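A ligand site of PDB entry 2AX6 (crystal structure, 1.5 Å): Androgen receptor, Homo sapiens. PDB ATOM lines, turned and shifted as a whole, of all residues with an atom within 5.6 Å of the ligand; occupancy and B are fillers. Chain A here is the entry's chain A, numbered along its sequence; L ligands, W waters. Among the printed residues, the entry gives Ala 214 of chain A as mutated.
The side-chain amide oxygen of Asn 42 is in hydrogen-bond range of an oxygen (O4) of the ligand.
OE1 of Gln 48 lies close to O1 of the ligand, at 2.5 Å.
O4 of the ligand is in hydrogen-bond range of N of Asn 42 (3.2 Å).
The backbone carbonyl oxygen (O) of Leu 41 sits close to an oxygen (O4) of the ligand.
O1 of the ligand is in hydrogen-bond range of NH2 of Arg 89, at 3.1 Å.
The backbone carbonyl oxygen (O) of Met 82 sits close to an oxygen (O2) of the ligand, at 3.0 Å.
A fluorine (F2) of the ligand lies close to the backbone NH of Val 83, at 3.2 Å.
A fluorine (F1) of the ligand sits close to the side-chain sulfur (SD) of Met 124, 3.7 Å away.
Residues that only touch the ligand: Leu 38 (3.97 Å), Leu 44 (3.6 Å), Gly 45 (3.9 Å), Met 79 (3.9 Å), Met 86 (3.1 Å), Phe 101 (3.3 Å), Leu 210 (3.3 Å), Ala 214 (3.8 Å) and Met 232 (3.7 Å).
Within 4 Å of the ligand: Leu 38, Leu 41, Asn 42, Leu 44, Gly 45, Gln 48, Met 79, Met 82, Val 83, Met 86, Arg 89, Phe 101, Met 124, Leu 210, Ala 214 and Met 232.
The nearest printed residue that does not touch the ligand is Phe 213 (4.2 Å).
Water W2 bridges the backbone carbonyl oxygen (O) of Leu 210 (2.9 Å) and an oxygen (O3) of the ligand (3.0 Å).
Water W1 lies within hydrogen-bond range of the guanidinium group of Arg 89, the backbone carbonyl oxygen of Met 82, an oxygen (O2) of the ligand and the side-chain amide nitrogen of Gln 48.
The side-chain amide nitrogen of Asn 42 sits close to the backbone carbonyl oxygen of Leu 38 (3.5 Å).
The side-chain sulfur (SD) of Met 82 sits at hydrogen-bond distance from the side-chain amide nitrogen (NE2) of Gln 48 (2.8 Å).
The side-chain amide oxygen of Asn 42 lies close to the side-chain sulfur of Met 232, at 3.6 Å.
The guanidinium group (NH2) of Arg 89 is in hydrogen-bond range of the backbone carbonyl oxygen (O) of Phe 101, at 3.1 Å.
The side-chain sulfur (SD) of Met 82 is in hydrogen-bond range of the indole nitrogen (NE1) of Trp 78.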
ATOM      1  N   LEU A  38      23.592 -16.755  -4.282  1.00  0.00           N
ATOM      2  CA  LEU A  38      23.894 -17.898  -5.139  1.00  0.00           C
ATOM      3  C   LEU A  38      22.872 -19.021  -4.997  1.00  0.00           C
ATOM      4  O   LEU A  38      22.582 -19.726  -5.959  1.00  0.00           O
ATOM      5  CB  LEU A  38      25.316 -18.397  -4.857  1.00  0.00           C
ATOM      6  CG  LEU A  38      26.367 -17.718  -5.750  1.00  0.00           C
ATOM      7  CD1 LEU A  38      26.130 -18.105  -7.203  1.00  0.00           C
ATOM      8  CD2 LEU A  38      26.304 -16.197  -5.609  1.00  0.00           C
ATOM      9  N   LEU A  41      20.262 -17.929  -7.268  1.00  0.00           N
ATOM     10  CA  LEU A  41      20.633 -18.080  -8.683  1.00  0.00           C
ATOM     11  C   LEU A  41      20.505 -19.549  -9.079  1.00  0.00           C
ATOM     12  O   LEU A  41      20.041 -19.869 -10.166  1.00  0.00           O
ATOM     13  CB  LEU A  41      22.068 -17.580  -8.928  1.00  0.00           C
ATOM     14  CG  LEU A  41      22.207 -16.066  -9.086  1.00  0.00           C
ATOM     15  CD1 LEU A  41      23.679 -15.668  -9.061  1.00  0.00           C
ATOM     16  CD2 LEU A  41      21.553 -15.614 -10.386  1.00  0.00           C
ATOM     17  N   ASN A  42      20.904 -20.448  -8.181  1.00  0.00           N
ATOM     18  CA  ASN A  42      20.812 -21.879  -8.471  1.00  0.00           C
ATOM     19  C   ASN A  42      19.365 -22.309  -8.591  1.00  0.00           C
ATOM     20  O   ASN A  42      19.015 -23.055  -9.484  1.00  0.00           O
ATOM     21  CB  ASN A  42      21.499 -22.714  -7.376  1.00  0.00           C
ATOM     22  CG  ASN A  42      23.010 -22.614  -7.428  1.00  0.00           C
ATOM     23  OD1 ASN A  42      23.589 -22.181  -8.425  1.00  0.00           O
ATOM     24  ND2 ASN A  42      23.661 -23.031  -6.353  1.00  0.00           N
ATOM     25  N   GLU A  43      18.515 -21.838  -7.674  1.00  0.00           N
ATOM     26  CA  GLU A  43      17.102 -22.200  -7.717  1.00  0.00           C
ATOM     27  C   GLU A  43      16.467 -21.630  -8.981  1.00  0.00           C
ATOM     28  O   GLU A  43      15.693 -22.313  -9.663  1.00  0.00           O
ATOM     29  CB  GLU A  43      16.371 -21.670  -6.477  1.00  0.00           C
ATOM     30  CG  GLU A  43      14.856 -21.863  -6.517  1.00  0.00           C
ATOM     31  CD  GLU A  43      14.424 -23.319  -6.553  1.00  0.00           C
ATOM     32  OE1 GLU A  43      13.256 -23.580  -6.892  1.00  0.00           O
ATOM     33  OE2 GLU A  43      15.244 -24.213  -6.231  1.00  0.00           O
ATOM     34  N   LEU A  44      16.798 -20.384  -9.296  1.00  0.00           N
ATOM     35  CA  LEU A  44      16.260 -19.754 -10.499  1.00  0.00           C
ATOM     36  C   LEU A  44      16.684 -20.572 -11.718  1.00  0.00           C
ATOM     37  O   LEU A  44      15.915 -20.767 -12.637  1.00  0.00           O
ATOM     38  CB  LEU A  44      16.767 -18.316 -10.642  1.00  0.00           C
ATOM     39  CG  LEU A  44      16.339 -17.601 -11.928  1.00  0.00           C
ATOM     40  CD1 LEU A  44      14.811 -17.521 -11.994  1.00  0.00           C
ATOM     41  CD2 LEU A  44      16.946 -16.217 -11.993  1.00  0.00           C
ATOM     42  N   GLY A  45      17.934 -21.045 -11.693  1.00  0.00           N
ATOM     43  CA  GLY A  45      18.432 -21.836 -12.804  1.00  0.00           C
ATOM     44  C   GLY A  45      17.637 -23.119 -12.974  1.00  0.00           C
ATOM     45  O   GLY A  45      17.295 -23.498 -14.093  1.00  0.00           O
ATOM     46  N   GLN A  48      14.250 -22.193 -14.381  1.00  0.00           N
ATOM     47  CA  GLN A  48      14.345 -21.823 -15.779  1.00  0.00           C
ATOM     48  C   GLN A  48      14.594 -23.031 -16.672  1.00  0.00           C
ATOM     49  O   GLN A  48      14.060 -23.099 -17.767  1.00  0.00           O
ATOM     50  CB  GLN A  48      15.440 -20.767 -15.977  1.00  0.00           C
ATOM     51  CG  GLN A  48      15.021 -19.398 -15.423  1.00  0.00           C
ATOM     52  CD  GLN A  48      16.029 -18.316 -15.682  1.00  0.00           C
ATOM     53  OE1 GLN A  48      15.741 -17.130 -15.494  1.00  0.00           O
ATOM     54  NE2 GLN A  48      17.226 -18.692 -16.111  1.00  0.00           N
ATOM     55  N   TRP A  78      21.848 -24.759 -22.580  1.00  0.00           N
ATOM     56  CA  TRP A  78      21.130 -24.153 -21.462  1.00  0.00           C
ATOM     57  C   TRP A  78      21.695 -22.817 -20.971  1.00  0.00           C
ATOM     58  O   TRP A  78      20.988 -21.808 -20.959  1.00  0.00           O
ATOM     59  CB  TRP A  78      21.055 -25.176 -20.321  1.00  0.00           C
ATOM     60  CG  TRP A  78      20.610 -24.639 -19.011  1.00  0.00           C
ATOM     61  CD1 TRP A  78      19.401 -24.070 -18.714  1.00  0.00           C
ATOM     62  CD2 TRP A  78      21.356 -24.654 -17.801  1.00  0.00           C
ATOM     63  NE1 TRP A  78      19.355 -23.741 -17.379  1.00  0.00           N
ATOM     64  CE2 TRP A  78      20.543 -24.087 -16.794  1.00  0.00           C
ATOM     65  CE3 TRP A  78      22.649 -25.101 -17.453  1.00  0.00           C
ATOM     66  CZ2 TRP A  78      20.979 -23.940 -15.469  1.00  0.00           C
ATOM     67  CZ3 TRP A  78      23.078 -24.946 -16.136  1.00  0.00           C
ATOM     68  CH2 TRP A  78      22.240 -24.376 -15.163  1.00  0.00           C
ATOM     69  N   MET A  79      22.969 -22.777 -20.584  1.00  0.00           N
ATOM     70  CA  MET A  79      23.540 -21.534 -20.082  1.00  0.00           C
ATOM     71  C   MET A  79      23.469 -20.399 -21.089  1.00  0.00           C
ATOM     72  O   MET A  79      23.071 -19.291 -20.755  1.00  0.00           O
ATOM     73  CB  MET A  79      24.998 -21.752 -19.644  1.00  0.00           C
ATOM     74  CG  MET A  79      25.630 -20.551 -18.905  1.00  0.00           C
ATOM     75  SD  MET A  79      24.826 -20.166 -17.328  1.00  0.00           S
ATOM     76  CE  MET A  79      25.442 -21.506 -16.303  1.00  0.00           C
ATOM     77  N   MET A  82      20.006 -19.042 -21.459  1.00  0.00           N
ATOM     78  CA  MET A  82      19.652 -18.240 -20.291  1.00  0.00           C
ATOM     79  C   MET A  82      20.313 -16.863 -20.374  1.00  0.00           C
ATOM     80  O   MET A  82      19.658 -15.845 -20.150  1.00  0.00           O
ATOM     81  CB  MET A  82      20.060 -18.931 -18.988  1.00  0.00           C
ATOM     82  CG  MET A  82      19.159 -20.089 -18.541  1.00  0.00           C
ATOM     83  SD  MET A  82      19.286 -20.441 -16.740  1.00  0.00           S
ATOM     84  CE  MET A  82      21.026 -20.754 -16.548  1.00  0.00           C
ATOM     85  N   VAL A  83      21.604 -16.830 -20.703  1.00  0.00           N
ATOM     86  CA  VAL A  83      22.337 -15.577 -20.811  1.00  0.00           C
ATOM     87  C   VAL A  83      21.699 -14.627 -21.821  1.00  0.00           C
ATOM     88  O   VAL A  83      21.507 -13.445 -21.550  1.00  0.00           O
ATOM     89  CB  VAL A  83      23.807 -15.817 -21.235  1.00  0.00           C
ATOM     90  CG1 VAL A  83      24.489 -14.487 -21.557  1.00  0.00           C
ATOM     91  CG2 VAL A  83      24.565 -16.518 -20.102  1.00  0.00           C
ATOM     92  N   MET A  86      18.286 -13.378 -20.578  1.00  0.00           N
ATOM     93  CA  MET A  86      18.460 -12.458 -19.457  1.00  0.00           C
ATOM     94  C   MET A  86      18.917 -11.094 -19.975  1.00  0.00           C
ATOM     95  O   MET A  86      18.456 -10.049 -19.520  1.00  0.00           O
ATOM     96  CB  MET A  86      19.466 -13.028 -18.461  1.00  0.00           C
ATOM     97  CG  MET A  86      19.486 -12.329 -17.118  1.00  0.00           C
ATOM     98  SD  MET A  86      20.500 -10.840 -17.093  1.00  0.00           S
ATOM     99  CE  MET A  86      22.108 -11.564 -17.014  1.00  0.00           C
ATOM    100  N   ARG A  89      15.892  -9.287 -21.297  1.00  0.00           N
ATOM    101  CA  ARG A  89      15.030  -8.820 -20.216  1.00  0.00           C
ATOM    102  C   ARG A  89      15.626  -7.572 -19.573  1.00  0.00           C
ATOM    103  O   ARG A  89      14.921  -6.618 -19.241  1.00  0.00           O
ATOM    104  CB  ARG A  89      14.866  -9.896 -19.126  1.00  0.00           C
ATOM    105  CG  ARG A  89      14.010 -11.095 -19.504  1.00  0.00           C
ATOM    106  CD  ARG A  89      13.615 -11.898 -18.265  1.00  0.00           C
ATOM    107  NE  ARG A  89      14.758 -12.494 -17.566  1.00  0.00           N
ATOM    108  CZ  ARG A  89      15.341 -13.640 -17.922  1.00  0.00           C
ATOM    109  NH1 ARG A  89      14.895 -14.318 -18.966  1.00  0.00           N
ATOM    110  NH2 ARG A  89      16.355 -14.113 -17.215  1.00  0.00           N
ATOM    111  N   PHE A 101      17.723 -10.833 -13.765  1.00  0.00           N
ATOM    112  CA  PHE A 101      17.681 -12.289 -13.748  1.00  0.00           C
ATOM    113  C   PHE A 101      16.230 -12.730 -13.595  1.00  0.00           C
ATOM    114  O   PHE A 101      15.774 -13.682 -14.236  1.00  0.00           O
ATOM    115  CB  PHE A 101      18.520 -12.864 -12.582  1.00  0.00           C
ATOM    116  CG  PHE A 101      20.012 -12.720 -12.769  1.00  0.00           C
ATOM    117  CD1 PHE A 101      20.691 -11.605 -12.271  1.00  0.00           C
ATOM    118  CD2 PHE A 101      20.740 -13.716 -13.404  1.00  0.00           C
ATOM    119  CE1 PHE A 101      22.075 -11.504 -12.404  1.00  0.00           C
ATOM    120  CE2 PHE A 101      22.126 -13.608 -13.545  1.00  0.00           C
ATOM    121  CZ  PHE A 101      22.794 -12.498 -13.042  1.00  0.00           C
ATOM    122  N   MET A 117      30.646 -12.833  -9.054  1.00  0.00           N
ATOM    123  CA  MET A 117      30.471 -13.092 -10.476  1.00  0.00           C
ATOM    124  C   MET A 117      30.555 -11.761 -11.201  1.00  0.00           C
ATOM    125  O   MET A 117      29.964 -11.594 -12.271  1.00  0.00           O
ATOM    126  CB  MET A 117      29.095 -13.696 -10.757  1.00  0.00           C
ATOM    127  CG  MET A 117      28.752 -14.908  -9.942  1.00  0.00           C
ATOM    128  SD  MET A 117      27.044 -15.363 -10.212  1.00  0.00           S
ATOM    129  CE  MET A 117      27.142 -16.050 -11.835  1.00  0.00           C
ATOM    130  N   MET A 124      27.640  -9.504 -19.302  1.00  0.00           N
ATOM    131  CA  MET A 124      26.231  -9.690 -19.617  1.00  0.00           C
ATOM    132  C   MET A 124      25.529  -8.333 -19.723  1.00  0.00           C
ATOM    133  O   MET A 124      24.582  -8.176 -20.500  1.00  0.00           O
ATOM    134  CB  MET A 124      25.561 -10.581 -18.551  1.00  0.00           C
ATOM    135  CG  MET A 124      26.093 -12.010 -18.569  1.00  0.00           C
ATOM    136  SD  MET A 124      25.062 -13.206 -17.684  1.00  0.00           S
ATOM    137  CE  MET A 124      25.618 -12.929 -15.994  1.00  0.00           C
ATOM    138  N   LEU A 210      30.602 -18.469 -17.319  1.00  0.00           N
ATOM    139  CA  LEU A 210      29.577 -18.838 -16.358  1.00  0.00           C
ATOM    140  C   LEU A 210      29.673 -20.338 -16.083  1.00  0.00           C
ATOM    141  O   LEU A 210      29.466 -20.795 -14.949  1.00  0.00           O
ATOM    142  CB  LEU A 210      28.195 -18.488 -16.887  1.00  0.00           C
ATOM    143  CG  LEU A 210      27.845 -17.003 -16.770  1.00  0.00           C
ATOM    144  CD1 LEU A 210      26.646 -16.679 -17.623  1.00  0.00           C
ATOM    145  CD2 LEU A 210      27.567 -16.679 -15.300  1.00  0.00           C
ATOM    146  N   PHE A 213      32.456 -20.824 -13.668  1.00  0.00           N
ATOM    147  CA  PHE A 213      32.060 -20.372 -12.354  1.00  0.00           C
ATOM    148  C   PHE A 213      31.123 -21.359 -11.666  1.00  0.00           C
ATOM    149  O   PHE A 213      31.305 -21.688 -10.497  1.00  0.00           O
ATOM    150  CB  PHE A 213      31.400 -18.991 -12.452  1.00  0.00           C
ATOM    151  CG  PHE A 213      30.871 -18.487 -11.158  1.00  0.00           C
ATOM    152  CD1 PHE A 213      29.567 -18.774 -10.765  1.00  0.00           C
ATOM    153  CD2 PHE A 213      31.681 -17.742 -10.306  1.00  0.00           C
ATOM    154  CE1 PHE A 213      29.076 -18.325  -9.541  1.00  0.00           C
ATOM    155  CE2 PHE A 213      31.199 -17.294  -9.080  1.00  0.00           C
ATOM    156  CZ  PHE A 213      29.898 -17.582  -8.701  1.00  0.00           C
ATOM    157  N   ALA A 214      30.128 -21.844 -12.397  1.00  0.00           N
ATOM    158  CA  ALA A 214      29.170 -22.795 -11.837  1.00  0.00           C
ATOM    159  C   ALA A 214      29.862 -24.091 -11.433  1.00  0.00           C
ATOM    160  O   ALA A 214      29.564 -24.666 -10.384  1.00  0.00           O
ATOM    161  CB  ALA A 214      28.067 -23.090 -12.846  1.00  0.00           C
ATOM    162  N   LEU A 217      31.977 -23.560  -8.314  1.00  0.00           N
ATOM    163  CA  LEU A 217      31.092 -23.411  -7.163  1.00  0.00           C
ATOM    164  C   LEU A 217      30.518 -24.746  -6.712  1.00  0.00           C
ATOM    165  O   LEU A 217      30.425 -25.018  -5.518  1.00  0.00           O
ATOM    166  CB  LEU A 217      29.955 -22.435  -7.491  1.00  0.00           C
ATOM    167  CG  LEU A 217      29.051 -22.076  -6.315  1.00  0.00           C
ATOM    168  CD1 LEU A 217      29.877 -21.481  -5.174  1.00  0.00           C
ATOM    169  CD2 LEU A 217      27.992 -21.082  -6.773  1.00  0.00           C
ATOM    170  N   PHE A 228      22.713 -26.752  -4.321  1.00  0.00           N
ATOM    171  CA  PHE A 228      22.501 -27.049  -5.735  1.00  0.00           C
ATOM    172  C   PHE A 228      21.348 -28.002  -6.013  1.00  0.00           C
ATOM    173  O   PHE A 228      21.312 -29.134  -5.508  1.00  0.00           O
ATOM    174  CB  PHE A 228      23.757 -27.627  -6.383  1.00  0.00           C
ATOM    175  CG  PHE A 228      24.786 -26.598  -6.730  1.00  0.00           C
ATOM    176  CD1 PHE A 228      25.608 -26.054  -5.754  1.00  0.00           C
ATOM    177  CD2 PHE A 228      24.924 -26.155  -8.043  1.00  0.00           C
ATOM    178  CE1 PHE A 228      26.552 -25.093  -6.079  1.00  0.00           C
ATOM    179  CE2 PHE A 228      25.863 -25.179  -8.384  1.00  0.00           C
ATOM    180  CZ  PHE A 228      26.680 -24.648  -7.394  1.00  0.00           C
ATOM    181  N   MET A 232      20.301 -29.289 -12.029  1.00  0.00           N
ATOM    182  CA  MET A 232      21.424 -28.407 -12.274  1.00  0.00           C
ATOM    183  C   MET A 232      22.739 -29.113 -11.941  1.00  0.00           C
ATOM    184  O   MET A 232      23.687 -29.083 -12.726  1.00  0.00           O
ATOM    185  CB  MET A 232      21.319 -27.133 -11.441  1.00  0.00           C
ATOM    186  CG  MET A 232      22.500 -26.201 -11.633  1.00  0.00           C
ATOM    187  SD  MET A 232      22.388 -24.662 -10.702  1.00  0.00           S
ATOM    188  CE  MET A 232      21.293 -23.732 -11.749  1.00  0.00           C
ATOM    189  N   ILE A 236      25.813 -29.744 -14.465  1.00  0.00           N
ATOM    190  CA  ILE A 236      27.107 -29.157 -14.142  1.00  0.00           C
ATOM    191  C   ILE A 236      28.222 -30.181 -13.939  1.00  0.00           C
ATOM    192  O   ILE A 236      29.378 -29.917 -14.273  1.00  0.00           O
ATOM    193  CB  ILE A 236      27.005 -28.265 -12.893  1.00  0.00           C
ATOM    194  CG1 ILE A 236      26.022 -27.123 -13.168  1.00  0.00           C
ATOM    195  CG2 ILE A 236      28.372 -27.695 -12.534  1.00  0.00           C
ATOM    196  CD1 ILE A 236      25.796 -26.195 -11.995  1.00  0.00           C
HETATM  197  F1  LIG L   1      23.654 -16.259 -16.179  1.00  0.00           F
HETATM  198  C1  LIG L   1      22.348 -16.302 -16.407  1.00  0.00           C
HETATM  199  F2  LIG L   1      22.174 -16.908 -17.581  1.00  0.00           F
HETATM  200  F3  LIG L   1      21.961 -15.034 -16.499  1.00  0.00           F
HETATM  201  C2  LIG L   1      21.594 -17.060 -15.295  1.00  0.00           C
HETATM  202  C3  LIG L   1      22.316 -17.851 -14.404  1.00  0.00           C
HETATM  203  C4  LIG L   1      20.214 -16.947 -15.096  1.00  0.00           C
HETATM  204  N1  LIG L   1      19.377 -16.363 -15.952  1.00  0.00           N
HETATM  205  O1  LIG L   1      18.015 -16.223 -15.620  1.00  0.00           O
HETATM  206  O2  LIG L   1      19.812 -15.807 -17.190  1.00  0.00           O
HETATM  207  C5  LIG L   1      19.613 -17.604 -14.023  1.00  0.00           C
HETATM  208  C6  LIG L   1      20.359 -18.384 -13.142  1.00  0.00           C
HETATM  209  C7  LIG L   1      21.725 -18.516 -13.337  1.00  0.00           C
HETATM  210  N2  LIG L   1      22.394 -19.301 -12.485  1.00  0.00           N
HETATM  211  C8  LIG L   1      23.700 -19.588 -12.520  1.00  0.00           C
HETATM  212  O3  LIG L   1      24.494 -19.154 -13.361  1.00  0.00           O
HETATM  213  C9  LIG L   1      24.165 -20.523 -11.407  1.00  0.00           C
HETATM  214  C10 LIG L   1      24.615 -21.847 -12.035  1.00  0.00           C
HETATM  215  C11 LIG L   1      25.333 -19.875 -10.664  1.00  0.00           C
HETATM  216  O4  LIG L   1      23.077 -20.756 -10.507  1.00  0.00           O
HETATM  217  O   HOH W   1      17.152 -16.464 -18.760  1.00  0.00           O
HETATM  218  O   HOH W   2      27.458 -19.630 -13.282  1.00  0.00           O
